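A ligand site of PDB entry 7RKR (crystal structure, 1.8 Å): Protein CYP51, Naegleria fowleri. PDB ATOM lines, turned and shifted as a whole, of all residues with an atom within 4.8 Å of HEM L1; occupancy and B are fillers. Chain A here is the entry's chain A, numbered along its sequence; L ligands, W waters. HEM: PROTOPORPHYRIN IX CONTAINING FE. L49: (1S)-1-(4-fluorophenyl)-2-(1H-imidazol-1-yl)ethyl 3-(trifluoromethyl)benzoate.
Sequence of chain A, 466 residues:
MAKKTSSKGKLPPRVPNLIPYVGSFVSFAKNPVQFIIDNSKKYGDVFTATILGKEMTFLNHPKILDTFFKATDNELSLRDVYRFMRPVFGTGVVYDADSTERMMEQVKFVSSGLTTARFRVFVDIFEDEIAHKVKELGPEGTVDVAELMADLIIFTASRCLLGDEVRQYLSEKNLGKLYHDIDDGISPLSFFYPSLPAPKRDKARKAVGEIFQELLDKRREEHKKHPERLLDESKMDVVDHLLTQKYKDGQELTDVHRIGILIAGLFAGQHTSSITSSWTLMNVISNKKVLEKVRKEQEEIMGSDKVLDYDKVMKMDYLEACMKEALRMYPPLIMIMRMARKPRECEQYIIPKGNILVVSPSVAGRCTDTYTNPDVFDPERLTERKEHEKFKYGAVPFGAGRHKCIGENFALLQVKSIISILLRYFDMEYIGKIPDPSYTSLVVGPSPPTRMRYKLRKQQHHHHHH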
ATOM      1  N   LEU A  78      14.667  -6.266  -4.145  1.00  0.00           N
ATOM      2  CA  LEU A  78      13.304  -6.344  -4.618  1.00  0.00           C
ATOM      3  C   LEU A  78      13.108  -5.616  -5.908  1.00  0.00           C
ATOM      4  O   LEU A  78      12.415  -6.088  -6.761  1.00  0.00           O
ATOM      5  CB  LEU A  78      12.398  -5.715  -3.632  1.00  0.00           C
ATOM      6  CG  LEU A  78      12.096  -6.584  -2.458  1.00  0.00           C
ATOM      7  CD1 LEU A  78      13.287  -6.475  -1.512  1.00  0.00           C
ATOM      8  CD2 LEU A  78      10.824  -6.151  -1.784  1.00  0.00           C
ATOM      9  N   TYR A  82      10.909  -7.016  -9.154  1.00  0.00           N
ATOM     10  CA  TYR A  82       9.527  -6.501  -9.307  1.00  0.00           C
ATOM     11  C   TYR A  82       9.368  -5.250 -10.161  1.00  0.00           C
ATOM     12  O   TYR A  82       8.222  -4.742 -10.321  1.00  0.00           O
ATOM     13  CB  TYR A  82       8.939  -6.269  -7.913  1.00  0.00           C
ATOM     14  CG  TYR A  82       8.920  -7.487  -7.038  1.00  0.00           C
ATOM     15  CD1 TYR A  82       8.717  -8.754  -7.592  1.00  0.00           C
ATOM     16  CD2 TYR A  82       8.982  -7.384  -5.648  1.00  0.00           C
ATOM     17  CE1 TYR A  82       8.580  -9.880  -6.801  1.00  0.00           C
ATOM     18  CE2 TYR A  82       8.838  -8.515  -4.831  1.00  0.00           C
ATOM     19  CZ  TYR A  82       8.641  -9.765  -5.425  1.00  0.00           C
ATOM     20  OH  TYR A  82       8.497 -10.918  -4.702  1.00  0.00           O
ATOM     21  N   TYR A  95       8.840  -0.229  -7.082  1.00  0.00           N
ATOM     22  CA  TYR A  95       9.962  -1.025  -7.541  1.00  0.00           C
ATOM     23  C   TYR A  95      10.746  -0.402  -8.710  1.00  0.00           C
ATOM     24  O   TYR A  95      11.849  -0.883  -8.993  1.00  0.00           O
ATOM     25  CB  TYR A  95       9.583  -2.486  -7.788  1.00  0.00           C
ATOM     26  CG  TYR A  95       8.886  -3.081  -6.550  1.00  0.00           C
ATOM     27  CD1 TYR A  95       9.532  -3.146  -5.328  1.00  0.00           C
ATOM     28  CD2 TYR A  95       7.557  -3.531  -6.605  1.00  0.00           C
ATOM     29  CE1 TYR A  95       8.900  -3.629  -4.199  1.00  0.00           C
ATOM     30  CE2 TYR A  95       6.937  -4.042  -5.464  1.00  0.00           C
ATOM     31  CZ  TYR A  95       7.609  -4.079  -4.280  1.00  0.00           C
ATOM     32  OH  TYR A  95       6.977  -4.562  -3.152  1.00  0.00           O
ATOM     33  N   MET A 103      11.610   4.508  -2.545  1.00  0.00           N
ATOM     34  CA  MET A 103      10.537   3.474  -2.465  1.00  0.00           C
ATOM     35  C   MET A 103       9.977   3.419  -1.058  1.00  0.00           C
ATOM     36  O   MET A 103       8.785   3.507  -0.833  1.00  0.00           O
ATOM     37  CB  MET A 103      11.107   2.104  -2.847  1.00  0.00           C
ATOM     38  CG  MET A 103      10.263   0.913  -2.392  1.00  0.00           C
ATOM     39  SD  MET A 103      10.729  -0.668  -3.169  1.00  0.00           S
ATOM     40  CE  MET A 103      12.432  -0.992  -2.673  1.00  0.00           C
ATOM     41  N   MET A 104      10.872   3.309  -0.093  1.00  0.00           N
ATOM     42  CA  MET A 104      10.486   3.372   1.313  1.00  0.00           C
ATOM     43  C   MET A 104       9.750   4.629   1.713  1.00  0.00           C
ATOM     44  O   MET A 104       8.807   4.546   2.475  1.00  0.00           O
ATOM     45  CB  MET A 104      11.689   3.078   2.228  1.00  0.00           C
ATOM     46  CG  MET A 104      12.101   1.595   2.137  1.00  0.00           C
ATOM     47  SD  MET A 104      10.753   0.389   2.537  1.00  0.00           S
ATOM     48  CE  MET A 104      10.756  -0.623   1.073  1.00  0.00           C
ATOM     49  N   VAL A 107       6.182   4.219   0.333  1.00  0.00           N
ATOM     50  CA  VAL A 107       5.405   3.299   1.138  1.00  0.00           C
ATOM     51  C   VAL A 107       4.868   4.011   2.340  1.00  0.00           C
ATOM     52  O   VAL A 107       3.671   3.907   2.647  1.00  0.00           O
ATOM     53  CB  VAL A 107       6.250   2.076   1.527  1.00  0.00           C
ATOM     54  CG1 VAL A 107       5.626   1.246   2.680  1.00  0.00           C
ATOM     55  CG2 VAL A 107       6.434   1.266   0.283  1.00  0.00           C
ATOM     56  N   VAL A 110       1.546   5.840   1.851  1.00  0.00           N
ATOM     57  CA  VAL A 110       0.332   5.002   1.897  1.00  0.00           C
ATOM     58  C   VAL A 110       0.011   4.623   3.394  1.00  0.00           C
ATOM     59  O   VAL A 110      -1.126   4.799   3.908  1.00  0.00           O
ATOM     60  CB  VAL A 110       0.476   3.765   0.994  1.00  0.00           C
ATOM     61  CG1 VAL A 110      -0.687   2.816   1.146  1.00  0.00           C
ATOM     62  CG2 VAL A 110       0.691   4.172  -0.477  1.00  0.00           C
ATOM     63  N   LEU A 114      -3.342   4.928   7.003  1.00  0.00           N
ATOM     64  CA  LEU A 114      -3.838   3.760   7.642  1.00  0.00           C
ATOM     65  C   LEU A 114      -3.657   3.887   9.154  1.00  0.00           C
ATOM     66  O   LEU A 114      -3.029   3.068   9.812  1.00  0.00           O
ATOM     67  CB  LEU A 114      -3.071   2.536   7.121  1.00  0.00           C
ATOM     68  CG  LEU A 114      -3.123   2.241   5.608  1.00  0.00           C
ATOM     69  CD1 LEU A 114      -2.245   1.024   5.294  1.00  0.00           C
ATOM     70  CD2 LEU A 114      -4.547   2.090   5.155  1.00  0.00           C
ATOM     71  N   LEU A 161      -8.860   4.684   0.947  1.00  0.00           N
ATOM     72  CA  LEU A 161      -7.582   5.213   0.583  1.00  0.00           C
ATOM     73  C   LEU A 161      -7.694   6.560  -0.059  1.00  0.00           C
ATOM     74  O   LEU A 161      -6.796   7.424   0.151  1.00  0.00           O
ATOM     75  CB  LEU A 161      -6.818   4.274  -0.326  1.00  0.00           C
ATOM     76  CG  LEU A 161      -6.501   2.935   0.318  1.00  0.00           C
ATOM     77  CD1 LEU A 161      -5.822   2.003  -0.690  1.00  0.00           C
ATOM     78  CD2 LEU A 161      -5.599   3.121   1.553  1.00  0.00           C
ATOM     79  N   GLY A 265      -1.315   1.502  -4.317  1.00  0.00           N
ATOM     80  CA  GLY A 265      -2.070   1.446  -3.074  1.00  0.00           C
ATOM     81  C   GLY A 265      -3.344   0.656  -3.269  1.00  0.00           C
ATOM     82  O   GLY A 265      -3.639  -0.202  -2.488  1.00  0.00           O
ATOM     83  N   ALA A 268      -2.616  -3.112  -3.928  1.00  0.00           N
ATOM     84  CA  ALA A 268      -2.371  -3.775  -2.619  1.00  0.00           C
ATOM     85  C   ALA A 268      -3.619  -3.871  -1.695  1.00  0.00           C
ATOM     86  O   ALA A 268      -3.771  -4.829  -1.027  1.00  0.00           O
ATOM     87  CB  ALA A 268      -1.200  -3.137  -1.869  1.00  0.00           C
ATOM     88  N   GLY A 269      -4.482  -2.864  -1.681  1.00  0.00           N
ATOM     89  CA  GLY A 269      -5.642  -2.799  -0.865  1.00  0.00           C
ATOM     90  C   GLY A 269      -6.848  -3.614  -1.293  1.00  0.00           C
ATOM     91  O   GLY A 269      -7.779  -3.796  -0.479  1.00  0.00           O
ATOM     92  N   THR A 272      -5.445  -9.059  -2.625  1.00  0.00           N
ATOM     93  CA  THR A 272      -5.142  -9.955  -1.539  1.00  0.00           C
ATOM     94  C   THR A 272      -6.254 -10.063  -0.480  1.00  0.00           C
ATOM     95  O   THR A 272      -6.511 -11.175  -0.052  1.00  0.00           O
ATOM     96  CB  THR A 272      -3.810  -9.663  -0.838  1.00  0.00           C
ATOM     97  OG1 THR A 272      -3.745  -8.302  -0.472  1.00  0.00           O
ATOM     98  CG2 THR A 272      -2.721  -9.970  -1.745  1.00  0.00           C
ATOM     99  N   SER A 273      -6.936  -8.959  -0.198  1.00  0.00           N
ATOM    100  CA  SER A 273      -8.031  -8.890   0.668  1.00  0.00           C
ATOM    101  C   SER A 273      -9.280  -9.590   0.131  1.00  0.00           C
ATOM    102  O   SER A 273      -9.866 -10.287   0.871  1.00  0.00           O
ATOM    103  CB  SER A 273      -8.413  -7.440   0.987  1.00  0.00           C
ATOM    104  OG  SER A 273      -7.484  -6.929   1.933  1.00  0.00           O
ATOM    105  N   THR A 276      -8.607 -13.354   0.191  1.00  0.00           N
ATOM    106  CA  THR A 276      -8.634 -13.868   1.554  1.00  0.00           C
ATOM    107  C   THR A 276     -10.048 -13.850   2.142  1.00  0.00           C
ATOM    108  O   THR A 276     -10.412 -14.762   2.810  1.00  0.00           O
ATOM    109  CB  THR A 276      -7.574 -13.147   2.407  1.00  0.00           C
ATOM    110  OG1 THR A 276      -6.306 -13.266   1.771  1.00  0.00           O
ATOM    111  CG2 THR A 276      -7.492 -13.759   3.783  1.00  0.00           C
ATOM    112  N   MET A 323      -9.319 -16.181   9.478  1.00  0.00           N
ATOM    113  CA  MET A 323      -8.621 -15.481   8.381  1.00  0.00           C
ATOM    114  C   MET A 323      -7.158 -15.897   8.299  1.00  0.00           C
ATOM    115  O   MET A 323      -6.689 -16.219   7.220  1.00  0.00           O
ATOM    116  CB  MET A 323      -8.693 -13.991   8.552  1.00  0.00           C
ATOM    117  CG  MET A 323      -7.849 -13.215   7.543  1.00  0.00           C
ATOM    118  SD  MET A 323      -8.239 -11.449   7.546  1.00  0.00           S
ATOM    119  CE  MET A 323      -6.897 -10.825   6.535  1.00  0.00           C
ATOM    120  N   LEU A 327      -5.154 -17.858   5.332  1.00  0.00           N
ATOM    121  CA  LEU A 327      -3.880 -17.412   4.844  1.00  0.00           C
ATOM    122  C   LEU A 327      -2.778 -18.484   4.858  1.00  0.00           C
ATOM    123  O   LEU A 327      -1.970 -18.517   3.936  1.00  0.00           O
ATOM    124  CB  LEU A 327      -3.377 -16.185   5.518  1.00  0.00           C
ATOM    125  CG  LEU A 327      -4.172 -14.933   5.157  1.00  0.00           C
ATOM    126  CD1 LEU A 327      -3.837 -13.848   6.166  1.00  0.00           C
ATOM    127  CD2 LEU A 327      -3.845 -14.480   3.729  1.00  0.00           C
ATOM    128  N   PRO A 332      -2.492 -15.575  -0.884  1.00  0.00           N
ATOM    129  CA  PRO A 332      -2.733 -15.061  -2.237  1.00  0.00           C
ATOM    130  C   PRO A 332      -1.438 -14.657  -2.966  1.00  0.00           C
ATOM    131  O   PRO A 332      -1.453 -14.534  -4.185  1.00  0.00           O
ATOM    132  CB  PRO A 332      -3.612 -13.832  -2.004  1.00  0.00           C
ATOM    133  CG  PRO A 332      -3.292 -13.430  -0.615  1.00  0.00           C
ATOM    134  CD  PRO A 332      -2.997 -14.678   0.161  1.00  0.00           C
ATOM    135  N   LEU A 333      -0.364 -14.443  -2.230  1.00  0.00           N
ATOM    136  CA  LEU A 333       0.959 -14.200  -2.787  1.00  0.00           C
ATOM    137  C   LEU A 333       1.764 -15.458  -2.485  1.00  0.00           C
ATOM    138  O   LEU A 333       2.176 -15.713  -1.309  1.00  0.00           O
ATOM    139  CB  LEU A 333       1.591 -12.988  -2.131  1.00  0.00           C
ATOM    140  CG  LEU A 333       0.885 -11.624  -2.278  1.00  0.00           C
ATOM    141  CD1 LEU A 333       1.793 -10.559  -1.710  1.00  0.00           C
ATOM    142  CD2 LEU A 333       0.546 -11.298  -3.711  1.00  0.00           C
ATOM    143  N   ILE A 336       7.493 -15.157  -2.831  1.00  0.00           N
ATOM    144  CA  ILE A 336       8.227 -13.962  -2.455  1.00  0.00           C
ATOM    145  C   ILE A 336       9.625 -14.048  -3.054  1.00  0.00           C
ATOM    146  O   ILE A 336      10.351 -15.060  -2.878  1.00  0.00           O
ATOM    147  CB  ILE A 336       8.340 -13.888  -0.914  1.00  0.00           C
ATOM    148  CG1 ILE A 336       7.039 -13.509  -0.282  1.00  0.00           C
ATOM    149  CG2 ILE A 336       9.374 -12.897  -0.414  1.00  0.00           C
ATOM    150  CD1 ILE A 336       7.084 -13.664   1.232  1.00  0.00           C
ATOM    151  N   ARG A 338      13.590 -12.330  -4.310  1.00  0.00           N
ATOM    152  CA  ARG A 338      14.691 -11.363  -4.252  1.00  0.00           C
ATOM    153  C   ARG A 338      15.809 -11.686  -5.266  1.00  0.00           C
ATOM    154  O   ARG A 338      16.171 -12.847  -5.392  1.00  0.00           O
ATOM    155  CB  ARG A 338      15.369 -11.399  -2.894  1.00  0.00           C
ATOM    156  CG  ARG A 338      14.463 -11.335  -1.696  1.00  0.00           C
ATOM    157  CD  ARG A 338      14.003  -9.895  -1.530  1.00  0.00           C
ATOM    158  NE  ARG A 338      13.269  -9.797  -0.288  1.00  0.00           N
ATOM    159  CZ  ARG A 338      11.956  -9.748  -0.159  1.00  0.00           C
ATOM    160  NH1 ARG A 338      11.158  -9.895  -1.235  1.00  0.00           N
ATOM    161  NH2 ARG A 338      11.443  -9.608   1.082  1.00  0.00           N
ATOM    162  N   VAL A 396       4.346 -17.094   7.255  1.00  0.00           N
ATOM    163  CA  VAL A 396       4.814 -15.872   6.582  1.00  0.00           C
ATOM    164  C   VAL A 396       3.831 -15.382   5.507  1.00  0.00           C
ATOM    165  O   VAL A 396       4.270 -15.006   4.450  1.00  0.00           O
ATOM    166  CB  VAL A 396       6.206 -16.125   5.948  1.00  0.00           C
ATOM    167  CG1 VAL A 396       7.268 -16.110   7.025  1.00  0.00           C
ATOM    168  CG2 VAL A 396       6.212 -17.413   5.114  1.00  0.00           C
ATOM    169  N   PRO A 397       2.510 -15.350   5.788  1.00  0.00           N
ATOM    170  CA  PRO A 397       1.614 -14.901   4.731  1.00  0.00           C
ATOM    171  C   PRO A 397       1.735 -13.392   4.452  1.00  0.00           C
ATOM    172  O   PRO A 397       1.394 -12.966   3.361  1.00  0.00           O
ATOM    173  CB  PRO A 397       0.248 -15.229   5.326  1.00  0.00           C
ATOM    174  CG  PRO A 397       0.425 -14.998   6.782  1.00  0.00           C
ATOM    175  CD  PRO A 397       1.785 -15.517   7.078  1.00  0.00           C
ATOM    176  N   PHE A 398       2.169 -12.623   5.452  1.00  0.00           N
ATOM    177  CA  PHE A 398       2.395 -11.181   5.334  1.00  0.00           C
ATOM    178  C   PHE A 398       3.920 -10.867   5.241  1.00  0.00           C
ATOM    179  O   PHE A 398       4.335  -9.723   5.317  1.00  0.00           O
ATOM    180  CB  PHE A 398       1.753 -10.416   6.501  1.00  0.00           C
ATOM    181  CG  PHE A 398       0.248 -10.364   6.476  1.00  0.00           C
ATOM    182  CD1 PHE A 398      -0.413  -9.492   5.631  1.00  0.00           C
ATOM    183  CD2 PHE A 398      -0.521 -11.186   7.310  1.00  0.00           C
ATOM    184  CE1 PHE A 398      -1.782  -9.440   5.617  1.00  0.00           C
ATOM    185  CE2 PHE A 398      -1.909 -11.145   7.273  1.00  0.00           C
ATOM    186  CZ  PHE A 398      -2.547 -10.235   6.465  1.00  0.00           C
ATOM    187  N   GLY A 399       4.751 -11.880   5.021  1.00  0.00           N
ATOM    188  CA  GLY A 399       6.182 -11.671   4.924  1.00  0.00           C
ATOM    189  C   GLY A 399       6.766 -11.494   6.303  1.00  0.00           C
ATOM    190  O   GLY A 399       6.173 -11.916   7.290  1.00  0.00           O
ATOM    191  N   HIS A 403      10.698  -5.912   4.844  1.00  0.00           N
ATOM    192  CA  HIS A 403       9.627  -5.677   3.866  1.00  0.00           C
ATOM    193  C   HIS A 403       8.284  -6.282   4.287  1.00  0.00           C
ATOM    194  O   HIS A 403       7.441  -6.554   3.458  1.00  0.00           O
ATOM    195  CB  HIS A 403      10.118  -6.145   2.503  1.00  0.00           C
ATOM    196  CG  HIS A 403      11.277  -5.346   1.990  1.00  0.00           C
ATOM    197  ND1 HIS A 403      11.157  -4.076   1.481  1.00  0.00           N
ATOM    198  CD2 HIS A 403      12.595  -5.630   1.981  1.00  0.00           C
ATOM    199  CE1 HIS A 403      12.341  -3.617   1.149  1.00  0.00           C
ATOM    200  NE2 HIS A 403      13.229  -4.531   1.468  1.00  0.00           N
ATOM    201  N   LYS A 404       8.118  -6.505   5.582  1.00  0.00           N
ATOM    202  CA  LYS A 404       6.879  -7.072   6.117  1.00  0.00           C
ATOM    203  C   LYS A 404       5.712  -6.163   5.737  1.00  0.00           C
ATOM    204  O   LYS A 404       5.870  -4.951   5.614  1.00  0.00           O
ATOM    205  CB  LYS A 404       6.970  -7.269   7.644  1.00  0.00           C
ATOM    206  CG  LYS A 404       5.840  -8.168   8.191  1.00  0.00           C
ATOM    207  CD  LYS A 404       6.026  -8.612   9.661  1.00  0.00           C
ATOM    208  CE  LYS A 404       4.807  -9.366  10.210  1.00  0.00           C
ATOM    209  NZ  LYS A 404       4.276 -10.418   9.307  1.00  0.00           N
ATOM    210  N   CYS A 405       4.575  -6.750   5.382  1.00  0.00           N
ATOM    211  CA  CYS A 405       3.415  -6.012   4.895  1.00  0.00           C
ATOM    212  C   CYS A 405       2.967  -4.938   5.841  1.00  0.00           C
ATOM    213  O   CYS A 405       2.629  -5.217   6.977  1.00  0.00           O
ATOM    214  CB  CYS A 405       2.230  -6.983   4.751  1.00  0.00           C
ATOM    215  SG  CYS A 405       0.790  -6.214   4.030  1.00  0.00           S
ATOM    216  N   ILE A 406       2.872  -3.712   5.354  1.00  0.00           N
ATOM    217  CA  ILE A 406       2.396  -2.606   6.171  1.00  0.00           C
ATOM    218  C   ILE A 406       0.899  -2.455   6.130  1.00  0.00           C
ATOM    219  O   ILE A 406       0.377  -1.682   6.891  1.00  0.00           O
ATOM    220  CB  ILE A 406       3.052  -1.238   5.784  1.00  0.00           C
ATOM    221  CG1 ILE A 406       2.733  -0.817   4.353  1.00  0.00           C
ATOM    222  CG2 ILE A 406       4.586  -1.322   6.081  1.00  0.00           C
ATOM    223  CD1 ILE A 406       1.690   0.259   4.169  1.00  0.00           C
ATOM    224  N   GLY A 407       0.252  -3.180   5.219  1.00  0.00           N
ATOM    225  CA  GLY A 407      -1.172  -3.231   5.108  1.00  0.00           C
ATOM    226  C   GLY A 407      -1.828  -4.265   6.002  1.00  0.00           C
ATOM    227  O   GLY A 407      -3.003  -4.432   5.883  1.00  0.00           O
ATOM    228  N   PHE A 410      -4.843  -3.126   8.209  1.00  0.00           N
ATOM    229  CA  PHE A 410      -5.957  -2.730   7.354  1.00  0.00           C
ATOM    230  C   PHE A 410      -6.645  -3.929   6.706  1.00  0.00           C
ATOM    231  O   PHE A 410      -7.861  -3.969   6.607  1.00  0.00           O
ATOM    232  CB  PHE A 410      -5.497  -1.754   6.278  1.00  0.00           C
ATOM    233  CG  PHE A 410      -6.566  -1.435   5.257  1.00  0.00           C
ATOM    234  CD1 PHE A 410      -7.657  -0.677   5.590  1.00  0.00           C
ATOM    235  CD2 PHE A 410      -6.501  -1.931   4.009  1.00  0.00           C
ATOM    236  CE1 PHE A 410      -8.659  -0.376   4.690  1.00  0.00           C
ATOM    237  CE2 PHE A 410      -7.500  -1.617   3.060  1.00  0.00           C
ATOM    238  CZ  PHE A 410      -8.560  -0.816   3.403  1.00  0.00           C
ATOM    239  N   ALA A 411      -5.854  -4.941   6.302  1.00  0.00           N
ATOM    240  CA  ALA A 411      -6.413  -6.084   5.643  1.00  0.00           C
ATOM    241  C   ALA A 411      -7.244  -6.922   6.628  1.00  0.00           C
ATOM    242  O   ALA A 411      -8.346  -7.347   6.308  1.00  0.00           O
ATOM    243  CB  ALA A 411      -5.347  -6.900   4.946  1.00  0.00           C
HETATM  244  CHA HEM L   1       4.278  -6.487   1.675  1.00  0.00           C
HETATM  245  CHB HEM L   1       0.851  -9.914   1.812  1.00  0.00           C
HETATM  246  CHC HEM L   1      -2.564  -6.509   2.157  1.00  0.00           C
HETATM  247  CHD HEM L   1       0.797  -3.127   1.339  1.00  0.00           C
HETATM  248  C1A HEM L   1       3.618  -7.689   1.725  1.00  0.00           C
HETATM  249  C2A HEM L   1       4.281  -8.960   1.712  1.00  0.00           C
HETATM  250  C3A HEM L   1       3.325  -9.910   1.768  1.00  0.00           C
HETATM  251  C4A HEM L   1       2.044  -9.264   1.731  1.00  0.00           C
HETATM  252  CMA HEM L   1       3.565 -11.404   1.706  1.00  0.00           C
HETATM  253  CAA HEM L   1       5.780  -9.179   1.680  1.00  0.00           C
HETATM  254  CBA HEM L   1       6.277  -9.079   0.189  1.00  0.00           C
HETATM  255  CGA HEM L   1       7.787  -9.219   0.078  1.00  0.00           C
HETATM  256  O1A HEM L   1       8.307  -9.134  -1.064  1.00  0.00           O
HETATM  257  O2A HEM L   1       8.542  -9.427   1.080  1.00  0.00           O
HETATM  258  C1B HEM L   1      -0.401  -9.299   2.002  1.00  0.00           C
HETATM  259  C2B HEM L   1      -1.570 -10.052   2.176  1.00  0.00           C
HETATM  260  C3B HEM L   1      -2.564  -9.126   2.263  1.00  0.00           C
HETATM  261  C4B HEM L   1      -1.909  -7.773   2.113  1.00  0.00           C
HETATM  262  CMB HEM L   1      -1.753 -11.561   2.226  1.00  0.00           C
HETATM  263  CAB HEM L   1      -4.012  -9.290   2.566  1.00  0.00           C
HETATM  264  CBB HEM L   1      -4.589 -10.308   3.224  1.00  0.00           C
HETATM  265  C1C HEM L   1      -1.929  -5.285   1.924  1.00  0.00           C
HETATM  266  C2C HEM L   1      -2.591  -4.049   1.923  1.00  0.00           C
HETATM  267  C3C HEM L   1      -1.636  -3.073   1.684  1.00  0.00           C
HETATM  268  C4C HEM L   1      -0.348  -3.749   1.560  1.00  0.00           C
HETATM  269  CMC HEM L   1      -4.096  -4.000   2.198  1.00  0.00           C
HETATM  270  CAC HEM L   1      -1.751  -1.594   1.532  1.00  0.00           C
HETATM  271  CBC HEM L   1      -2.887  -0.929   1.496  1.00  0.00           C
HETATM  272  C1D HEM L   1       2.014  -3.824   1.415  1.00  0.00           C
HETATM  273  C2D HEM L   1       3.209  -3.114   1.263  1.00  0.00           C
HETATM  274  C3D HEM L   1       4.196  -4.012   1.382  1.00  0.00           C
HETATM  275  C4D HEM L   1       3.555  -5.310   1.546  1.00  0.00           C
HETATM  276  CMD HEM L   1       3.395  -1.637   1.065  1.00  0.00           C
HETATM  277  CAD HEM L   1       5.693  -3.682   1.396  1.00  0.00           C
HETATM  278  CBD HEM L   1       6.472  -4.198   0.191  1.00  0.00           C
HETATM  279  CGD HEM L   1       7.912  -3.680   0.195  1.00  0.00           C
HETATM  280  O1D HEM L   1       8.419  -3.194   1.243  1.00  0.00           O
HETATM  281  O2D HEM L   1       8.560  -3.738  -0.899  1.00  0.00           O
HETATM  282  NA  HEM L   1       2.257  -7.925   1.754  1.00  0.00           N
HETATM  283  NB  HEM L   1      -0.621  -7.944   1.968  1.00  0.00           N
HETATM  284  NC  HEM L   1      -0.579  -5.029   1.662  1.00  0.00           N
HETATM  285  ND  HEM L   1       2.204  -5.176   1.538  1.00  0.00           N
HETATM  286 FE   HEM L   1       0.856  -6.485   1.731  1.00  0.00          FE
HETATM  287  F3  L49 L   2       1.075   0.798  -2.595  1.00  0.00           F
HETATM  288  C15 L49 L   2       2.344   0.822  -2.326  1.00  0.00           C
HETATM  289  F1  L49 L   2       2.884   1.749  -3.058  1.00  0.00           F
HETATM  290  F2  L49 L   2       2.516   1.170  -1.073  1.00  0.00           F
HETATM  291  C14 L49 L   2       2.937  -0.547  -2.596  1.00  0.00           C
HETATM  292  C13 L49 L   2       2.159  -1.568  -3.139  1.00  0.00           C
HETATM  293  C16 L49 L   2       4.269  -0.697  -2.266  1.00  0.00           C
HETATM  294  C17 L49 L   2       4.902  -1.936  -2.484  1.00  0.00           C
HETATM  295  C18 L49 L   2       4.122  -2.982  -2.987  1.00  0.00           C
HETATM  296  C   L49 L   2       2.786  -2.800  -3.334  1.00  0.00           C
HETATM  297  C1  L49 L   2       2.037  -3.943  -3.937  1.00  0.00           C
HETATM  298  O   L49 L   2       0.943  -3.845  -4.386  1.00  0.00           O
HETATM  299  O1  L49 L   2       2.691  -5.172  -3.989  1.00  0.00           O
HETATM  300  C2  L49 L   2       2.091  -6.295  -4.581  1.00  0.00           C
HETATM  301  C9  L49 L   2       2.082  -7.415  -3.556  1.00  0.00           C
HETATM  302  N   L49 L   2       1.306  -7.109  -2.347  1.00  0.00           N
HETATM  303  C12 L49 L   2       1.760  -6.904  -1.121  1.00  0.00           C
HETATM  304  N1  L49 L   2       0.745  -6.752  -0.230  1.00  0.00           N
HETATM  305  C11 L49 L   2      -0.398  -6.786  -0.960  1.00  0.00           C
HETATM  306  C10 L49 L   2      -0.066  -7.047  -2.285  1.00  0.00           C
HETATM  307  C3  L49 L   2       2.963  -6.708  -5.716  1.00  0.00           C
HETATM  308  C8  L49 L   2       2.448  -6.949  -6.997  1.00  0.00           C
HETATM  309  C7  L49 L   2       3.234  -7.345  -8.078  1.00  0.00           C
HETATM  310  C6  L49 L   2       4.612  -7.454  -7.832  1.00  0.00           C
HETATM  311  F   L49 L   2       5.477  -7.839  -8.760  1.00  0.00           F
HETATM  312  C5  L49 L   2       5.121  -7.194  -6.564  1.00  0.00           C
HETATM  313  C4  L49 L   2       4.331  -6.799  -5.537  1.00  0.00           C
HETATM  314  O   HOH W   1       6.541  -7.287  -2.641  1.00  0.00           O
HETATM  315  O   HOH W   2       8.775  -9.691   3.672  1.00  0.00           O
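Residues that only touch HEM L1: Thr 272 (3.1 Å), Pro 397 (3.1 Å), Ala 268 (3.3 Å), Leu 78 (3.4 Å), Ile 406 (3.5 Å), Phe 398 (3.5 Å), Gly 407 (3.5 Å), Met 104 (3.5 Å), Gly 399 (3.6 Å), Ala 411 (3.6 Å), Gly 269 (3.6 Å), Phe 410 (3.7 Å), Leu 333 (3.7 Å), Thr 276 (3.7 Å), Pro 332 (3.7 Å), Tyr 82 (3.9 Å), Ile 336 (3.9 Å), Leu 327 (3.9 Å) and Val 107 (3.99 Å). Hydrophobic or aromatic side chains within 4 Å of HEM L1: Leu 78, Tyr 82, Tyr 95, Met 104, Val 107, Ala 268, Leu 327, Pro 332, Leu 333, Ile 336, Phe 398, His 403, Ile 406, Phe 410 and Ala 411.
Water W2 lies within hydrogen-bond range of O2A of HEM L1 (2.6 Å) and O of His 403 (3.4 Å). Water W1 bridges the side-chain hydroxyl (OH) of Tyr 95 and an oxygen (O1A) of HEM L1.
The backbone NH of Cys 405 lies within hydrogen-bond range of the backbone carbonyl oxygen of Phe 398 (3.0 Å). N of Gly 407 lies close to SG of Cys 405 (3.3 Å). O of Thr 272 sits at hydrogen-bond distance from OG1 of Thr 276, at 2.8 Å. NZ of Lys 404 sits at hydrogen-bond distance from O of Gly 399.
FE of HEM L1 is bound by N1 of L49 L2 (2.0 Å).
The side-chain sulfur (SG) of Cys 405 binds an iron atom (FE) of HEM L1. The side-chain hydroxyl (OH) of Tyr 95 is in hydrogen-bond range of an oxygen (O2D) of HEM L1 (2.9 Å). ND1 of His 403 sits at hydrogen-bond distance from O1D of HEM L1 (2.9 Å). The guanidinium group (NH2) of Arg 338 lies within salt-bridge range of an oxygen (O2A) of HEM L1, at 2.9 Å.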
